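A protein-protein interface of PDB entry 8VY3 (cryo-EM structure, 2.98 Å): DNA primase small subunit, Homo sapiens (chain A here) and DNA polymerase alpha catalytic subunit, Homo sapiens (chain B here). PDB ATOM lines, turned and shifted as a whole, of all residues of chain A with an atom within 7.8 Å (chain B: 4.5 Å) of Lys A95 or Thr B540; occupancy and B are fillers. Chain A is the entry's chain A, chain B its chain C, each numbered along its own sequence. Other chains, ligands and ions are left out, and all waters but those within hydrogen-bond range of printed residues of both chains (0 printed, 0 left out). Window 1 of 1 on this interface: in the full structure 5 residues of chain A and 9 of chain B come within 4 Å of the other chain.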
ATOM      1  N   HIS A  86       2.588   3.815 -31.671  1.00  0.00           N
ATOM      2  CA  HIS A  86       2.571   4.725 -32.804  1.00  0.00           C
ATOM      3  C   HIS A  86       2.619   3.905 -34.082  1.00  0.00           C
ATOM      4  O   HIS A  86       3.041   2.746 -34.073  1.00  0.00           O
ATOM      5  CB  HIS A  86       3.747   5.707 -32.757  1.00  0.00           C
ATOM      6  CG  HIS A  86       3.799   6.530 -31.509  1.00  0.00           C
ATOM      7  ND1 HIS A  86       2.677   6.826 -30.764  1.00  0.00           N
ATOM      8  CD2 HIS A  86       4.840   7.109 -30.866  1.00  0.00           C
ATOM      9  CE1 HIS A  86       3.024   7.559 -29.722  1.00  0.00           C
ATOM     10  NE2 HIS A  86       4.331   7.745 -29.760  1.00  0.00           N
ATOM     11  N   HIS A  91       7.418   6.070 -37.097  1.00  0.00           N
ATOM     12  CA  HIS A  91       8.151   5.897 -35.850  1.00  0.00           C
ATOM     13  C   HIS A  91       9.326   6.855 -35.712  1.00  0.00           C
ATOM     14  O   HIS A  91       9.742   7.139 -34.583  1.00  0.00           O
ATOM     15  CB  HIS A  91       8.645   4.455 -35.715  1.00  0.00           C
ATOM     16  CG  HIS A  91       9.680   4.068 -36.723  1.00  0.00           C
ATOM     17  ND1 HIS A  91       9.532   4.301 -38.073  1.00  0.00           N
ATOM     18  CD2 HIS A  91      10.879   3.457 -36.577  1.00  0.00           C
ATOM     19  CE1 HIS A  91      10.594   3.850 -38.714  1.00  0.00           C
ATOM     20  NE2 HIS A  91      11.428   3.334 -37.829  1.00  0.00           N
ATOM     21  N   ASN A  92       9.874   7.352 -36.824  1.00  0.00           N
ATOM     22  CA  ASN A  92      10.922   8.365 -36.738  1.00  0.00           C
ATOM     23  C   ASN A  92      10.370   9.692 -36.239  1.00  0.00           C
ATOM     24  O   ASN A  92      11.133  10.546 -35.778  1.00  0.00           O
ATOM     25  CB  ASN A  92      11.592   8.549 -38.098  1.00  0.00           C
ATOM     26  CG  ASN A  92      12.603   7.465 -38.403  1.00  0.00           C
ATOM     27  OD1 ASN A  92      13.324   7.007 -37.519  1.00  0.00           O
ATOM     28  ND2 ASN A  92      12.663   7.049 -39.662  1.00  0.00           N
ATOM     29  N   THR A  93       9.052   9.880 -36.325  1.00  0.00           N
ATOM     30  CA  THR A  93       8.436  11.110 -35.844  1.00  0.00           C
ATOM     31  C   THR A  93       8.623  11.276 -34.341  1.00  0.00           C
ATOM     32  O   THR A  93       8.892  12.382 -33.860  1.00  0.00           O
ATOM     33  CB  THR A  93       6.950  11.116 -36.208  1.00  0.00           C
ATOM     34  OG1 THR A  93       6.797  11.414 -37.602  1.00  0.00           O
ATOM     35  CG2 THR A  93       6.186  12.142 -35.386  1.00  0.00           C
ATOM     36  N   VAL A  94       8.493  10.191 -33.585  1.00  0.00           N
ATOM     37  CA  VAL A  94       8.508  10.259 -32.129  1.00  0.00           C
ATOM     38  C   VAL A  94       9.940  10.188 -31.608  1.00  0.00           C
ATOM     39  O   VAL A  94      10.865   9.816 -32.338  1.00  0.00           O
ATOM     40  CB  VAL A  94       7.638   9.143 -31.524  1.00  0.00           C
ATOM     41  CG1 VAL A  94       8.409   7.835 -31.465  1.00  0.00           C
ATOM     42  CG2 VAL A  94       7.121   9.550 -30.151  1.00  0.00           C
ATOM     43  N   LYS A  95      10.127  10.553 -30.341  1.00  0.00           N
ATOM     44  CA  LYS A  95      11.442  10.543 -29.720  1.00  0.00           C
ATOM     45  C   LYS A  95      11.926   9.113 -29.495  1.00  0.00           C
ATOM     46  O   LYS A  95      11.140   8.170 -29.372  1.00  0.00           O
ATOM     47  CB  LYS A  95      11.403  11.311 -28.399  1.00  0.00           C
ATOM     48  CG  LYS A  95      12.757  11.770 -27.886  1.00  0.00           C
ATOM     49  CD  LYS A  95      12.606  12.957 -26.951  1.00  0.00           C
ATOM     50  CE  LYS A  95      11.630  12.663 -25.836  1.00  0.00           C
ATOM     51  NZ  LYS A  95      11.272  13.899 -25.091  1.00  0.00           N
ATOM     52  N   LEU A  96      13.249   8.962 -29.438  1.00  0.00           N
ATOM     53  CA  LEU A  96      13.892   7.659 -29.279  1.00  0.00           C
ATOM     54  C   LEU A  96      13.574   7.121 -27.889  1.00  0.00           C
ATOM     55  O   LEU A  96      14.063   7.638 -26.882  1.00  0.00           O
ATOM     56  CB  LEU A  96      15.396   7.773 -29.499  1.00  0.00           C
ATOM     57  CG  LEU A  96      16.051   6.664 -30.323  1.00  0.00           C
ATOM     58  CD1 LEU A  96      15.597   6.728 -31.770  1.00  0.00           C
ATOM     59  CD2 LEU A  96      17.564   6.758 -30.231  1.00  0.00           C
ATOM     60  N   GLY A  97      12.752   6.075 -27.835  1.00  0.00           N
ATOM     61  CA  GLY A  97      12.391   5.459 -26.574  1.00  0.00           C
ATOM     62  C   GLY A  97      10.895   5.370 -26.352  1.00  0.00           C
ATOM     63  O   GLY A  97      10.436   4.622 -25.486  1.00  0.00           O
ATOM     64  N   ALA A  98      10.126   6.139 -27.121  1.00  0.00           N
ATOM     65  CA  ALA A  98       8.673   6.139 -27.013  1.00  0.00           C
ATOM     66  C   ALA A  98       7.996   5.179 -27.982  1.00  0.00           C
ATOM     67  O   ALA A  98       6.770   5.043 -27.936  1.00  0.00           O
ATOM     68  CB  ALA A  98       8.126   7.554 -27.236  1.00  0.00           C
ATOM     69  N   PHE A  99       8.754   4.515 -28.850  1.00  0.00           N
ATOM     70  CA  PHE A  99       8.213   3.562 -29.809  1.00  0.00           C
ATOM     71  C   PHE A  99       8.504   2.150 -29.315  1.00  0.00           C
ATOM     72  O   PHE A  99       9.662   1.719 -29.306  1.00  0.00           O
ATOM     73  CB  PHE A  99       8.821   3.786 -31.193  1.00  0.00           C
ATOM     74  CG  PHE A  99       8.197   2.953 -32.276  1.00  0.00           C
ATOM     75  CD1 PHE A  99       6.905   3.203 -32.701  1.00  0.00           C
ATOM     76  CD2 PHE A  99       8.911   1.932 -32.879  1.00  0.00           C
ATOM     77  CE1 PHE A  99       6.335   2.442 -33.698  1.00  0.00           C
ATOM     78  CE2 PHE A  99       8.345   1.172 -33.880  1.00  0.00           C
ATOM     79  CZ  PHE A  99       7.057   1.427 -34.290  1.00  0.00           C
ATOM     80  N   GLN A 100       7.457   1.433 -28.914  1.00  0.00           N
ATOM     81  CA  GLN A 100       7.634   0.116 -28.324  1.00  0.00           C
ATOM     82  C   GLN A 100       6.393  -0.724 -28.584  1.00  0.00           C
ATOM     83  O   GLN A 100       5.280  -0.205 -28.688  1.00  0.00           O
ATOM     84  CB  GLN A 100       7.913   0.221 -26.821  1.00  0.00           C
ATOM     85  CG  GLN A 100       6.845   0.979 -26.054  1.00  0.00           C
ATOM     86  CD  GLN A 100       7.327   1.449 -24.697  1.00  0.00           C
ATOM     87  OE1 GLN A 100       8.511   1.355 -24.381  1.00  0.00           O
ATOM     88  NE2 GLN A 100       6.407   1.960 -23.888  1.00  0.00           N
ATOM     89  N   ALA B 103      14.388  18.599 -31.174  1.00  0.00           N
ATOM     90  CA  ALA B 103      14.297  17.903 -29.897  1.00  0.00           C
ATOM     91  C   ALA B 103      14.299  18.847 -28.701  1.00  0.00           C
ATOM     92  O   ALA B 103      15.011  18.598 -27.726  1.00  0.00           O
ATOM     93  CB  ALA B 103      15.452  16.912 -29.763  1.00  0.00           C
ATOM     94  N   GLU B 111       9.942  14.852 -34.077  1.00  0.00           N
ATOM     95  CA  GLU B 111      11.396  14.819 -33.965  1.00  0.00           C
ATOM     96  C   GLU B 111      12.074  14.590 -35.308  1.00  0.00           C
ATOM     97  O   GLU B 111      13.306  14.530 -35.366  1.00  0.00           O
ATOM     98  CB  GLU B 111      11.830  13.745 -32.969  1.00  0.00           C
ATOM     99  CG  GLU B 111      11.831  14.221 -31.526  1.00  0.00           C
ATOM    100  CD  GLU B 111      13.136  13.925 -30.814  1.00  0.00           C
ATOM    101  OE1 GLU B 111      13.989  13.224 -31.395  1.00  0.00           O
ATOM    102  OE2 GLU B 111      13.310  14.399 -29.673  1.00  0.00           O
ATOM    103  N   TYR B 464      19.715  19.889 -37.390  1.00  0.00           N
ATOM    104  CA  TYR B 464      18.746  20.100 -36.323  1.00  0.00           C
ATOM    105  C   TYR B 464      18.149  21.498 -36.415  1.00  0.00           C
ATOM    106  O   TYR B 464      18.760  22.403 -36.992  1.00  0.00           O
ATOM    107  CB  TYR B 464      19.398  19.911 -34.954  1.00  0.00           C
ATOM    108  CG  TYR B 464      19.250  18.526 -34.376  1.00  0.00           C
ATOM    109  CD1 TYR B 464      20.028  17.476 -34.837  1.00  0.00           C
ATOM    110  CD2 TYR B 464      18.338  18.271 -33.366  1.00  0.00           C
ATOM    111  CE1 TYR B 464      19.897  16.213 -34.313  1.00  0.00           C
ATOM    112  CE2 TYR B 464      18.201  17.009 -32.836  1.00  0.00           C
ATOM    113  CZ  TYR B 464      18.982  15.984 -33.313  1.00  0.00           C
ATOM    114  OH  TYR B 464      18.849  14.721 -32.788  1.00  0.00           O
ATOM    115  N   CYS B 538      20.368  13.568 -22.345  1.00  0.00           N
ATOM    116  CA  CYS B 538      20.479  14.455 -23.498  1.00  0.00           C
ATOM    117  C   CYS B 538      19.098  15.008 -23.815  1.00  0.00           C
ATOM    118  O   CYS B 538      18.094  14.622 -23.210  1.00  0.00           O
ATOM    119  CB  CYS B 538      21.072  13.732 -24.706  1.00  0.00           C
ATOM    120  SG  CYS B 538      21.212  14.752 -26.191  1.00  0.00           S
ATOM    121  N   PHE B 539      19.061  15.934 -24.770  1.00  0.00           N
ATOM    122  CA  PHE B 539      17.818  16.488 -25.287  1.00  0.00           C
ATOM    123  C   PHE B 539      17.030  15.484 -26.112  1.00  0.00           C
ATOM    124  O   PHE B 539      15.798  15.468 -26.032  1.00  0.00           O
ATOM    125  CB  PHE B 539      18.117  17.720 -26.144  1.00  0.00           C
ATOM    126  CG  PHE B 539      18.740  18.851 -25.386  1.00  0.00           C
ATOM    127  CD1 PHE B 539      18.048  19.493 -24.376  1.00  0.00           C
ATOM    128  CD2 PHE B 539      20.027  19.263 -25.677  1.00  0.00           C
ATOM    129  CE1 PHE B 539      18.626  20.533 -23.683  1.00  0.00           C
ATOM    130  CE2 PHE B 539      20.609  20.298 -24.986  1.00  0.00           C
ATOM    131  CZ  PHE B 539      19.908  20.935 -23.991  1.00  0.00           C
ATOM    132  N   THR B 540      17.715  14.638 -26.882  1.00  0.00           N
ATOM    133  CA  THR B 540      17.058  13.731 -27.812  1.00  0.00           C
ATOM    134  C   THR B 540      16.818  12.349 -27.221  1.00  0.00           C
ATOM    135  O   THR B 540      16.470  11.428 -27.967  1.00  0.00           O
ATOM    136  CB  THR B 540      17.890  13.589 -29.089  1.00  0.00           C
ATOM    137  OG1 THR B 540      18.957  12.663 -28.859  1.00  0.00           O
ATOM    138  CG2 THR B 540      18.483  14.926 -29.481  1.00  0.00           C
ATOM    139  N   THR B 541      16.997  12.171 -25.916  1.00  0.00           N
ATOM    140  CA  THR B 541      16.951  10.855 -25.295  1.00  0.00           C
ATOM    141  C   THR B 541      15.991  10.785 -24.116  1.00  0.00           C
ATOM    142  O   THR B 541      15.305   9.775 -23.933  1.00  0.00           O
ATOM    143  CB  THR B 541      18.373  10.460 -24.865  1.00  0.00           C
ATOM    144  OG1 THR B 541      19.086   9.940 -25.992  1.00  0.00           O
ATOM    145  CG2 THR B 541      18.348   9.416 -23.792  1.00  0.00           C
ATOM    146  N   VAL B 542      15.894  11.846 -23.327  1.00  0.00           N
ATOM    147  CA  VAL B 542      15.053  11.842 -22.135  1.00  0.00           C
ATOM    148  C   VAL B 542      13.613  12.173 -22.508  1.00  0.00           C
ATOM    149  O   VAL B 542      13.322  13.213 -23.105  1.00  0.00           O
ATOM    150  CB  VAL B 542      15.601  12.830 -21.087  1.00  0.00           C
ATOM    151  CG1 VAL B 542      14.632  12.971 -19.928  1.00  0.00           C
ATOM    152  CG2 VAL B 542      16.956  12.370 -20.592  1.00  0.00           C
ATOM    153  N   GLN B 543      12.699  11.277 -22.141  1.00  0.00           N
ATOM    154  CA  GLN B 543      11.267  11.490 -22.333  1.00  0.00           C
ATOM    155  C   GLN B 543      10.772  12.407 -21.221  1.00  0.00           C
ATOM    156  O   GLN B 543      10.907  12.087 -20.037  1.00  0.00           O
ATOM    157  CB  GLN B 543      10.514  10.162 -22.320  1.00  0.00           C
ATOM    158  CG  GLN B 543      10.235   9.574 -23.690  1.00  0.00           C
ATOM    159  CD  GLN B 543      11.432   8.841 -24.259  1.00  0.00           C
ATOM    160  OE1 GLN B 543      11.818   7.783 -23.764  1.00  0.00           O
ATOM    161  NE2 GLN B 543      12.023   9.397 -25.309  1.00  0.00           N
ATOM    162  N   ARG B 544      10.191  13.541 -21.599  1.00  0.00           N
ATOM    163  CA  ARG B 544       9.831  14.573 -20.639  1.00  0.00           C
ATOM    164  C   ARG B 544       8.425  15.076 -20.929  1.00  0.00           C
ATOM    165  O   ARG B 544       7.781  14.671 -21.899  1.00  0.00           O
ATOM    166  CB  ARG B 544      10.853  15.716 -20.666  1.00  0.00           C
ATOM    167  CG  ARG B 544      11.109  16.276 -22.051  1.00  0.00           C
ATOM    168  CD  ARG B 544      12.317  17.190 -22.054  1.00  0.00           C
ATOM    169  NE  ARG B 544      12.598  17.725 -23.380  1.00  0.00           N
ATOM    170  CZ  ARG B 544      13.719  17.502 -24.052  1.00  0.00           C
ATOM    171  NH1 ARG B 544      14.662  16.707 -23.577  1.00  0.00           N
ATOM    172  NH2 ARG B 544      13.896  18.087 -25.232  1.00  0.00           N
ATOM    173  N   GLY B 572      23.649  10.203 -27.140  1.00  0.00           N
ATOM    174  CA  GLY B 572      22.978  11.362 -27.690  1.00  0.00           C
ATOM    175  C   GLY B 572      23.976  12.371 -28.229  1.00  0.00           C
ATOM    176  O   GLY B 572      25.167  12.088 -28.364  1.00  0.00           O
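O of Thr A93 lies within hydrogen-bond range of N of Glu B111, at 2.7 Å.
The side-chain amino group of Lys A95 sits at hydrogen-bond distance from the backbone carbonyl oxygen of Val B542, 2.9 Å away.
The backbone carbonyl oxygen of Leu A96 sits at hydrogen-bond distance from the side-chain amide nitrogen of Gln B543 (3.1 Å).
The backbone carbonyl oxygen of Ala B103 sits at hydrogen-bond distance from the guanidinium group of Arg B544 (2.8 Å).
SG of Cys B538 sits close to N of Thr B540.
The backbone carbonyl oxygen (O) of Phe B539 sits at hydrogen-bond distance from the guanidinium group (NH1) of Arg B544, at 3.0 Å.
Among the printed residues, merely in contact across the chains: Lys A95 with Glu B111 (3.2 Å), Lys A95 with Gln B543 (3.3 Å), Gly A97 with Gln B543 (3.7 Å), Lys A95 with Arg B544 (3.7 Å), Lys A95 with Thr B540 (3.7 Å) and Leu A96 with Thr B541 (3.8 Å).
Lys A95 touches five residues of chain B.
Printed residues of chain A within 4 Å of Thr B540: Lys A95.
Of the printed residues of chain B, Thr A93 touches Glu B111 (2.7 Å).
Printed residues of chain A within 4 Å of Arg B544: Lys A95.
Of the printed residues of chain B, Leu A96 touches Thr B541 (3.8 Å) and Gln B543 (3.1 Å).
Gln A100 touches none of the printed residues of chain B.
Cys B538 touches none of the printed residues of chain A.
The nearest residue of chain A that does not touch Thr B540 is Leu A96 (4.1 Å).
Of the 11 printed residues of chain B, 6 touch a printed residue of chain A.
Printed residues of chain B that touch a printed residue of chain A: Glu B111, Thr B540, Thr B541, Val B542, Gln B543 and Arg B544.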
